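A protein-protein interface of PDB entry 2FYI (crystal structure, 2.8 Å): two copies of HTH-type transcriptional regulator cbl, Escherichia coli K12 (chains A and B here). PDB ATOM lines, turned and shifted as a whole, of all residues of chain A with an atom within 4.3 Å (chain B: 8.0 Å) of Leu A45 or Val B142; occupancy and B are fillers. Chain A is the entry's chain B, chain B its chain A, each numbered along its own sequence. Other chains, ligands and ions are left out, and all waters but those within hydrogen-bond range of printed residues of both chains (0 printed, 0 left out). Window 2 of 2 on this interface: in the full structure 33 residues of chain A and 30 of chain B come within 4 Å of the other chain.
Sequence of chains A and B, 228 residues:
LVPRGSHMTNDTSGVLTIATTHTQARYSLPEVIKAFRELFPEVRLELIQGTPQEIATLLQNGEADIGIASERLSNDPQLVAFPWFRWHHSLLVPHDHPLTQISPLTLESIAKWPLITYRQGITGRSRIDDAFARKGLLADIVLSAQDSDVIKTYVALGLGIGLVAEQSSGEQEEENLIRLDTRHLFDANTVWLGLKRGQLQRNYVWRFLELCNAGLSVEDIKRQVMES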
ATOM      1  N   LEU A  16       3.463  16.012  -7.470  1.00  0.00           N
ATOM      2  CA  LEU A  16       3.469  15.998  -8.924  1.00  0.00           C
ATOM      3  C   LEU A  16       4.493  17.006  -9.373  1.00  0.00           C
ATOM      4  O   LEU A  16       4.342  18.188  -9.096  1.00  0.00           O
ATOM      5  CB  LEU A  16       2.108  16.401  -9.446  1.00  0.00           C
ATOM      6  CG  LEU A  16       2.169  16.685 -10.926  1.00  0.00           C
ATOM      7  CD1 LEU A  16       2.480  15.395 -11.652  1.00  0.00           C
ATOM      8  CD2 LEU A  16       0.854  17.316 -11.404  1.00  0.00           C
ATOM      9  N   ILE A  18       6.269  18.975 -12.356  1.00  0.00           N
ATOM     10  CA  ILE A  18       6.151  19.316 -13.744  1.00  0.00           C
ATOM     11  C   ILE A  18       7.373  20.100 -14.162  1.00  0.00           C
ATOM     12  O   ILE A  18       7.796  21.022 -13.469  1.00  0.00           O
ATOM     13  CB  ILE A  18       4.882  20.158 -13.964  1.00  0.00           C
ATOM     14  CG1 ILE A  18       3.679  19.310 -13.665  1.00  0.00           C
ATOM     15  CG2 ILE A  18       4.777  20.676 -15.359  1.00  0.00           C
ATOM     16  CD1 ILE A  18       2.440  20.124 -13.568  1.00  0.00           C
ATOM     17  N   ILE A  33      -3.419  24.529 -13.399  1.00  0.00           N
ATOM     18  CA  ILE A  33      -2.994  24.360 -12.019  1.00  0.00           C
ATOM     19  C   ILE A  33      -4.133  24.662 -11.058  1.00  0.00           C
ATOM     20  O   ILE A  33      -4.433  23.849 -10.203  1.00  0.00           O
ATOM     21  CB  ILE A  33      -1.752  25.154 -11.728  1.00  0.00           C
ATOM     22  CG1 ILE A  33      -0.582  24.383 -12.298  1.00  0.00           C
ATOM     23  CG2 ILE A  33      -1.541  25.264 -10.250  1.00  0.00           C
ATOM     24  CD1 ILE A  33       0.602  25.227 -12.662  1.00  0.00           C
ATOM     25  N   ARG A  37      -5.444  21.928  -8.356  1.00  0.00           N
ATOM     26  CA  ARG A  37      -5.436  22.089  -6.918  1.00  0.00           C
ATOM     27  C   ARG A  37      -6.825  21.872  -6.275  1.00  0.00           C
ATOM     28  O   ARG A  37      -6.917  21.397  -5.159  1.00  0.00           O
ATOM     29  CB  ARG A  37      -4.847  23.445  -6.526  1.00  0.00           C
ATOM     30  CG  ARG A  37      -3.577  23.841  -7.281  1.00  0.00           C
ATOM     31  CD  ARG A  37      -2.219  23.356  -6.685  1.00  0.00           C
ATOM     32  NE  ARG A  37      -1.683  24.348  -5.755  1.00  0.00           N
ATOM     33  CZ  ARG A  37      -1.394  24.125  -4.474  1.00  0.00           C
ATOM     34  NH1 ARG A  37      -0.954  25.142  -3.738  1.00  0.00           N
ATOM     35  NH2 ARG A  37      -1.528  22.913  -3.936  1.00  0.00           N
ATOM     36  N   VAL A  43      -2.496  16.943  -2.895  1.00  0.00           N
ATOM     37  CA  VAL A  43      -1.311  16.631  -3.695  1.00  0.00           C
ATOM     38  C   VAL A  43      -0.434  17.855  -3.814  1.00  0.00           C
ATOM     39  O   VAL A  43      -0.889  18.897  -4.268  1.00  0.00           O
ATOM     40  CB  VAL A  43      -1.656  16.258  -5.150  1.00  0.00           C
ATOM     41  CG1 VAL A  43      -0.397  16.047  -5.954  1.00  0.00           C
ATOM     42  CG2 VAL A  43      -2.539  15.053  -5.223  1.00  0.00           C
ATOM     43  N   ARG A  44       0.831  17.733  -3.432  1.00  0.00           N
ATOM     44  CA  ARG A  44       1.774  18.818  -3.585  1.00  0.00           C
ATOM     45  C   ARG A  44       2.186  18.930  -5.045  1.00  0.00           C
ATOM     46  O   ARG A  44       2.627  17.973  -5.679  1.00  0.00           O
ATOM     47  CB  ARG A  44       2.997  18.575  -2.711  1.00  0.00           C
ATOM     48  CG  ARG A  44       4.201  19.450  -3.001  1.00  0.00           C
ATOM     49  CD  ARG A  44       5.409  18.910  -2.280  1.00  0.00           C
ATOM     50  NE  ARG A  44       6.595  19.637  -2.688  1.00  0.00           N
ATOM     51  CZ  ARG A  44       7.114  20.692  -2.067  1.00  0.00           C
ATOM     52  NH1 ARG A  44       8.192  21.248  -2.577  1.00  0.00           N
ATOM     53  NH2 ARG A  44       6.582  21.197  -0.955  1.00  0.00           N
ATOM     54  N   LEU A  45       2.061  20.122  -5.578  1.00  0.00           N
ATOM     55  CA  LEU A  45       2.540  20.399  -6.913  1.00  0.00           C
ATOM     56  C   LEU A  45       3.873  21.190  -6.903  1.00  0.00           C
ATOM     57  O   LEU A  45       3.991  22.176  -6.206  1.00  0.00           O
ATOM     58  CB  LEU A  45       1.449  21.161  -7.642  1.00  0.00           C
ATOM     59  CG  LEU A  45       1.723  21.919  -8.933  1.00  0.00           C
ATOM     60  CD1 LEU A  45       2.582  21.134  -9.895  1.00  0.00           C
ATOM     61  CD2 LEU A  45       0.369  22.191  -9.551  1.00  0.00           C
ATOM     62  N   GLU A  46       4.876  20.731  -7.654  1.00  0.00           N
ATOM     63  CA  GLU A  46       6.164  21.448  -7.847  1.00  0.00           C
ATOM     64  C   GLU A  46       6.468  21.731  -9.307  1.00  0.00           C
ATOM     65  O   GLU A  46       6.270  20.867 -10.153  1.00  0.00           O
ATOM     66  CB  GLU A  46       7.296  20.575  -7.430  1.00  0.00           C
ATOM     67  CG  GLU A  46       7.309  20.253  -6.028  1.00  0.00           C
ATOM     68  CD  GLU A  46       8.318  19.172  -5.802  1.00  0.00           C
ATOM     69  OE1 GLU A  46       8.736  18.597  -6.847  1.00  0.00           O
ATOM     70  OE2 GLU A  46       8.703  18.902  -4.623  1.00  0.00           O
ATOM     71  N   LEU A  47       6.982  22.910  -9.618  1.00  0.00           N
ATOM     72  CA  LEU A  47       7.408  23.195 -10.998  1.00  0.00           C
ATOM     73  C   LEU A  47       8.870  23.487 -11.113  1.00  0.00           C
ATOM     74  O   LEU A  47       9.445  24.175 -10.276  1.00  0.00           O
ATOM     75  CB  LEU A  47       6.776  24.456 -11.540  1.00  0.00           C
ATOM     76  CG  LEU A  47       5.296  24.684 -11.781  1.00  0.00           C
ATOM     77  CD1 LEU A  47       5.199  25.070 -13.273  1.00  0.00           C
ATOM     78  CD2 LEU A  47       4.518  23.447 -11.493  1.00  0.00           C
ATOM     79  N   TRP B 113       7.641  28.595   4.788  1.00  0.00           N
ATOM     80  CA  TRP B 113       6.685  28.681   3.671  1.00  0.00           C
ATOM     81  C   TRP B 113       7.238  28.117   2.382  1.00  0.00           C
ATOM     82  O   TRP B 113       8.465  28.023   2.216  1.00  0.00           O
ATOM     83  CB  TRP B 113       6.297  30.118   3.440  1.00  0.00           C
ATOM     84  CG  TRP B 113       5.858  30.747   4.675  1.00  0.00           C
ATOM     85  CD1 TRP B 113       6.648  31.229   5.720  1.00  0.00           C
ATOM     86  CD2 TRP B 113       4.526  30.968   5.047  1.00  0.00           C
ATOM     87  NE1 TRP B 113       5.844  31.731   6.717  1.00  0.00           N
ATOM     88  CE2 TRP B 113       4.540  31.575   6.330  1.00  0.00           C
ATOM     89  CE3 TRP B 113       3.314  30.708   4.426  1.00  0.00           C
ATOM     90  CZ2 TRP B 113       3.399  31.930   6.978  1.00  0.00           C
ATOM     91  CZ3 TRP B 113       2.188  31.028   5.073  1.00  0.00           C
ATOM     92  CH2 TRP B 113       2.224  31.653   6.341  1.00  0.00           C
ATOM     93  N   PRO B 114       6.347  27.716   1.460  1.00  0.00           N
ATOM     94  CA  PRO B 114       6.783  27.300   0.114  1.00  0.00           C
ATOM     95  C   PRO B 114       7.552  28.415  -0.621  1.00  0.00           C
ATOM     96  O   PRO B 114       7.022  29.487  -0.764  1.00  0.00           O
ATOM     97  CB  PRO B 114       5.439  26.996  -0.594  1.00  0.00           C
ATOM     98  CG  PRO B 114       4.509  26.667   0.509  1.00  0.00           C
ATOM     99  CD  PRO B 114       4.889  27.583   1.632  1.00  0.00           C
ATOM    100  N   LEU B 115       8.780  28.192  -1.066  1.00  0.00           N
ATOM    101  CA  LEU B 115       9.489  29.257  -1.787  1.00  0.00           C
ATOM    102  C   LEU B 115       9.426  29.123  -3.280  1.00  0.00           C
ATOM    103  O   LEU B 115       9.458  28.003  -3.833  1.00  0.00           O
ATOM    104  CB  LEU B 115      10.945  29.289  -1.459  1.00  0.00           C
ATOM    105  CG  LEU B 115      11.152  29.755  -0.045  1.00  0.00           C
ATOM    106  CD1 LEU B 115      12.653  30.043   0.173  1.00  0.00           C
ATOM    107  CD2 LEU B 115      10.271  30.985   0.217  1.00  0.00           C
ATOM    108  N   ILE B 116       9.366  30.276  -3.937  1.00  0.00           N
ATOM    109  CA  ILE B 116       9.440  30.334  -5.368  1.00  0.00           C
ATOM    110  C   ILE B 116      10.615  31.219  -5.649  1.00  0.00           C
ATOM    111  O   ILE B 116      10.593  32.408  -5.373  1.00  0.00           O
ATOM    112  CB  ILE B 116       8.196  30.949  -5.965  1.00  0.00           C
ATOM    113  CG1 ILE B 116       6.965  30.248  -5.439  1.00  0.00           C
ATOM    114  CG2 ILE B 116       8.226  30.875  -7.487  1.00  0.00           C
ATOM    115  CD1 ILE B 116       5.754  31.006  -5.792  1.00  0.00           C
ATOM    116  N   THR B 117      11.670  30.633  -6.182  1.00  0.00           N
ATOM    117  CA  THR B 117      12.889  31.393  -6.360  1.00  0.00           C
ATOM    118  C   THR B 117      13.741  30.865  -7.497  1.00  0.00           C
ATOM    119  O   THR B 117      13.348  29.911  -8.172  1.00  0.00           O
ATOM    120  CB  THR B 117      13.689  31.481  -5.074  1.00  0.00           C
ATOM    121  OG1 THR B 117      14.551  32.607  -5.168  1.00  0.00           O
ATOM    122  CG2 THR B 117      14.507  30.254  -4.861  1.00  0.00           C
ATOM    123  N   ALA B 139      15.725  25.449   2.255  1.00  0.00           N
ATOM    124  CA  ALA B 139      14.486  26.108   1.871  1.00  0.00           C
ATOM    125  C   ALA B 139      13.624  25.094   1.130  1.00  0.00           C
ATOM    126  O   ALA B 139      14.140  24.188   0.484  1.00  0.00           O
ATOM    127  CB  ALA B 139      14.754  27.305   1.008  1.00  0.00           C
ATOM    128  N   ASP B 140      12.310  25.225   1.276  1.00  0.00           N
ATOM    129  CA  ASP B 140      11.371  24.479   0.475  1.00  0.00           C
ATOM    130  C   ASP B 140      11.179  25.142  -0.886  1.00  0.00           C
ATOM    131  O   ASP B 140      10.393  26.074  -1.036  1.00  0.00           O
ATOM    132  CB  ASP B 140      10.005  24.423   1.143  1.00  0.00           C
ATOM    133  CG  ASP B 140       9.002  23.645   0.296  1.00  0.00           C
ATOM    134  OD1 ASP B 140       9.380  23.294  -0.865  1.00  0.00           O
ATOM    135  OD2 ASP B 140       7.866  23.367   0.771  1.00  0.00           O
ATOM    136  N   ILE B 141      11.879  24.660  -1.889  1.00  0.00           N
ATOM    137  CA  ILE B 141      11.700  25.200  -3.212  1.00  0.00           C
ATOM    138  C   ILE B 141      10.513  24.511  -3.869  1.00  0.00           C
ATOM    139  O   ILE B 141      10.569  23.326  -4.217  1.00  0.00           O
ATOM    140  CB  ILE B 141      12.892  24.926  -4.050  1.00  0.00           C
ATOM    141  CG1 ILE B 141      14.156  25.435  -3.343  1.00  0.00           C
ATOM    142  CG2 ILE B 141      12.670  25.526  -5.393  1.00  0.00           C
ATOM    143  CD1 ILE B 141      14.285  26.904  -3.289  1.00  0.00           C
ATOM    144  N   VAL B 142       9.424  25.242  -4.045  1.00  0.00           N
ATOM    145  CA  VAL B 142       8.262  24.638  -4.640  1.00  0.00           C
ATOM    146  C   VAL B 142       8.234  24.983  -6.133  1.00  0.00           C
ATOM    147  O   VAL B 142       7.543  24.340  -6.911  1.00  0.00           O
ATOM    148  CB  VAL B 142       7.002  25.114  -3.918  1.00  0.00           C
ATOM    149  CG1 VAL B 142       6.501  26.374  -4.549  1.00  0.00           C
ATOM    150  CG2 VAL B 142       5.962  24.082  -3.989  1.00  0.00           C
ATOM    151  N   LEU B 143       8.976  26.009  -6.524  1.00  0.00           N
ATOM    152  CA  LEU B 143       9.162  26.304  -7.921  1.00  0.00           C
ATOM    153  C   LEU B 143      10.528  26.897  -8.119  1.00  0.00           C
ATOM    154  O   LEU B 143      10.893  27.863  -7.461  1.00  0.00           O
ATOM    155  CB  LEU B 143       8.097  27.265  -8.459  1.00  0.00           C
ATOM    156  CG  LEU B 143       8.137  27.634  -9.962  1.00  0.00           C
ATOM    157  CD1 LEU B 143       6.830  28.212 -10.402  1.00  0.00           C
ATOM    158  CD2 LEU B 143       9.232  28.615 -10.312  1.00  0.00           C
ATOM    159  N   SER B 144      11.299  26.318  -9.032  1.00  0.00           N
ATOM    160  CA  SER B 144      12.630  26.840  -9.261  1.00  0.00           C
ATOM    161  C   SER B 144      12.632  27.470 -10.644  1.00  0.00           C
ATOM    162  O   SER B 144      12.279  26.835 -11.633  1.00  0.00           O
ATOM    163  CB  SER B 144      13.697  25.770  -9.083  1.00  0.00           C
ATOM    164  OG  SER B 144      14.027  25.205 -10.319  1.00  0.00           O
ATOM    165  N   ALA B 145      12.989  28.748 -10.678  1.00  0.00           N
ATOM    166  CA  ALA B 145      12.715  29.610 -11.813  1.00  0.00           C
ATOM    167  C   ALA B 145      13.998  30.012 -12.545  1.00  0.00           C
ATOM    168  O   ALA B 145      15.067  30.113 -11.951  1.00  0.00           O
ATOM    169  CB  ALA B 145      11.959  30.856 -11.334  1.00  0.00           C
ATOM    170  N   TYR B 154       3.575  32.958 -10.102  1.00  0.00           N
ATOM    171  CA  TYR B 154       3.191  31.886  -9.192  1.00  0.00           C
ATOM    172  C   TYR B 154       2.917  32.398  -7.783  1.00  0.00           C
ATOM    173  O   TYR B 154       2.153  31.769  -7.023  1.00  0.00           O
ATOM    174  CB  TYR B 154       4.131  30.655  -9.302  1.00  0.00           C
ATOM    175  CG  TYR B 154       3.757  29.958 -10.547  1.00  0.00           C
ATOM    176  CD1 TYR B 154       4.384  30.262 -11.755  1.00  0.00           C
ATOM    177  CD2 TYR B 154       2.668  29.130 -10.569  1.00  0.00           C
ATOM    178  CE1 TYR B 154       3.961  29.668 -12.951  1.00  0.00           C
ATOM    179  CE2 TYR B 154       2.223  28.552 -11.753  1.00  0.00           C
ATOM    180  CZ  TYR B 154       2.869  28.815 -12.938  1.00  0.00           C
ATOM    181  OH  TYR B 154       2.391  28.233 -14.112  1.00  0.00           O
ATOM    182  N   LEU B 157      -0.490  33.552  -8.119  1.00  0.00           N
ATOM    183  CA  LEU B 157      -1.400  32.431  -8.215  1.00  0.00           C
ATOM    184  C   LEU B 157      -1.715  31.805  -6.877  1.00  0.00           C
ATOM    185  O   LEU B 157      -2.738  31.162  -6.742  1.00  0.00           O
ATOM    186  CB  LEU B 157      -0.786  31.352  -9.073  1.00  0.00           C
ATOM    187  CG  LEU B 157      -1.812  30.382  -9.623  1.00  0.00           C
ATOM    188  CD1 LEU B 157      -2.619  31.103 -10.675  1.00  0.00           C
ATOM    189  CD2 LEU B 157      -1.098  29.210 -10.251  1.00  0.00           C
ATOM    190  N   GLY B 158      -0.837  31.943  -5.891  1.00  0.00           N
ATOM    191  CA  GLY B 158      -1.058  31.292  -4.632  1.00  0.00           C
ATOM    192  C   GLY B 158      -0.115  30.158  -4.299  1.00  0.00           C
ATOM    193  O   GLY B 158      -0.116  29.657  -3.177  1.00  0.00           O
ATOM    194  N   LEU B 159       0.727  29.749  -5.239  1.00  0.00           N
ATOM    195  CA  LEU B 159       1.620  28.616  -5.012  1.00  0.00           C
ATOM    196  C   LEU B 159       2.578  28.726  -3.819  1.00  0.00           C
ATOM    197  O   LEU B 159       2.962  27.681  -3.283  1.00  0.00           O
ATOM    198  CB  LEU B 159       2.435  28.375  -6.252  1.00  0.00           C
ATOM    199  CG  LEU B 159       3.076  27.004  -6.364  1.00  0.00           C
ATOM    200  CD1 LEU B 159       2.000  25.931  -6.581  1.00  0.00           C
ATOM    201  CD2 LEU B 159       4.070  27.027  -7.517  1.00  0.00           C
ATOM    202  N   GLY B 160       2.959  29.954  -3.421  1.00  0.00           N
ATOM    203  CA  GLY B 160       4.005  30.198  -2.411  1.00  0.00           C
ATOM    204  C   GLY B 160       4.529  31.647  -2.351  1.00  0.00           C
ATOM    205  O   GLY B 160       3.986  32.545  -2.988  1.00  0.00           O
ATOM    206  N   ILE B 161       5.571  31.918  -1.589  1.00  0.00           N
ATOM    207  CA  ILE B 161       6.139  33.264  -1.595  1.00  0.00           C
ATOM    208  C   ILE B 161       7.430  33.321  -2.430  1.00  0.00           C
ATOM    209  O   ILE B 161       8.021  32.281  -2.754  1.00  0.00           O
ATOM    210  CB  ILE B 161       6.458  33.730  -0.176  1.00  0.00           C
ATOM    211  CG1 ILE B 161       7.550  32.845   0.420  1.00  0.00           C
ATOM    212  CG2 ILE B 161       5.218  33.714   0.669  1.00  0.00           C
ATOM    213  CD1 ILE B 161       7.669  32.907   1.889  1.00  0.00           C
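Hydrophobic or aromatic side chains of chain A within 4 Å of the printed part of chain B: Ile A33 and Leu A47.
Tyr B154 touches Ile A33 (OH to CD1, 3.8 Å).
Leu B157 touches Ile A33 (CD2 to CG2, 3.97 Å).
Arg A44 touches Ile B141.
CG2 of Val B142 touches NH1 of Arg A44 (3.9 Å).
Val B142 touches Leu A45.
Val B142 touches Glu A46 (O to CA, 3.3 Å).
Leu A47 touches Leu B143.
NH1 of Arg A44 is in salt-bridge range of OD1 of Asp B140 (2.9 Å).
The backbone carbonyl oxygen (O) of Val B142 sits at hydrogen-bond distance from the backbone NH (N) of Leu A47, 3.1 Å away.
N of Ser B144 lies within hydrogen-bond range of O of Leu A47 (3.1 Å).
Printed residues of chain B within 4 Å of Leu A45: Val B142 (3.5 Å).
Printed residues of chain A within 4 Å of Val B142: Arg A44, Leu A45, Glu A46 and Leu A47.
Printed residues of chain A within 4 Å of Leu B143: Leu A47 (3.2 Å).
Of the printed residues of chain B, Ile A33 touches Tyr B154 and Leu B157.
Of the printed residues of chain A, Leu B157 touches Ile A33.
Gly B160 touches none of the printed residues of chain A.
Leu A16 touches none of the printed residues of chain B.
The nearest residue of chain B that does not touch Leu A45 is Leu B159 (4.3 Å).
The nearest printed residue of chain A that does not touch Ser B144 is Glu A46 (6.7 Å).
N of Leu B143 lies within hydrogen-bond range of O of Leu B115.
The backbone NH (N) of Thr B117 is in hydrogen-bond range of the backbone carbonyl oxygen (O) of Leu B143, at 3.1 Å.
O of Tyr B154 sits at hydrogen-bond distance from N of Leu B159 (3.0 Å).
The backbone NH (N) of Leu A16 is in hydrogen-bond range of the backbone carbonyl oxygen (O) of Arg A44 (2.8 Å).
The backbone NH of Glu A46 is in hydrogen-bond range of the backbone carbonyl oxygen of Leu A16, 3.0 Å away.
NE of Arg A44 is in salt-bridge range of OE2 of Glu A46, at 3.0 Å.
No position is printed for both chains.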
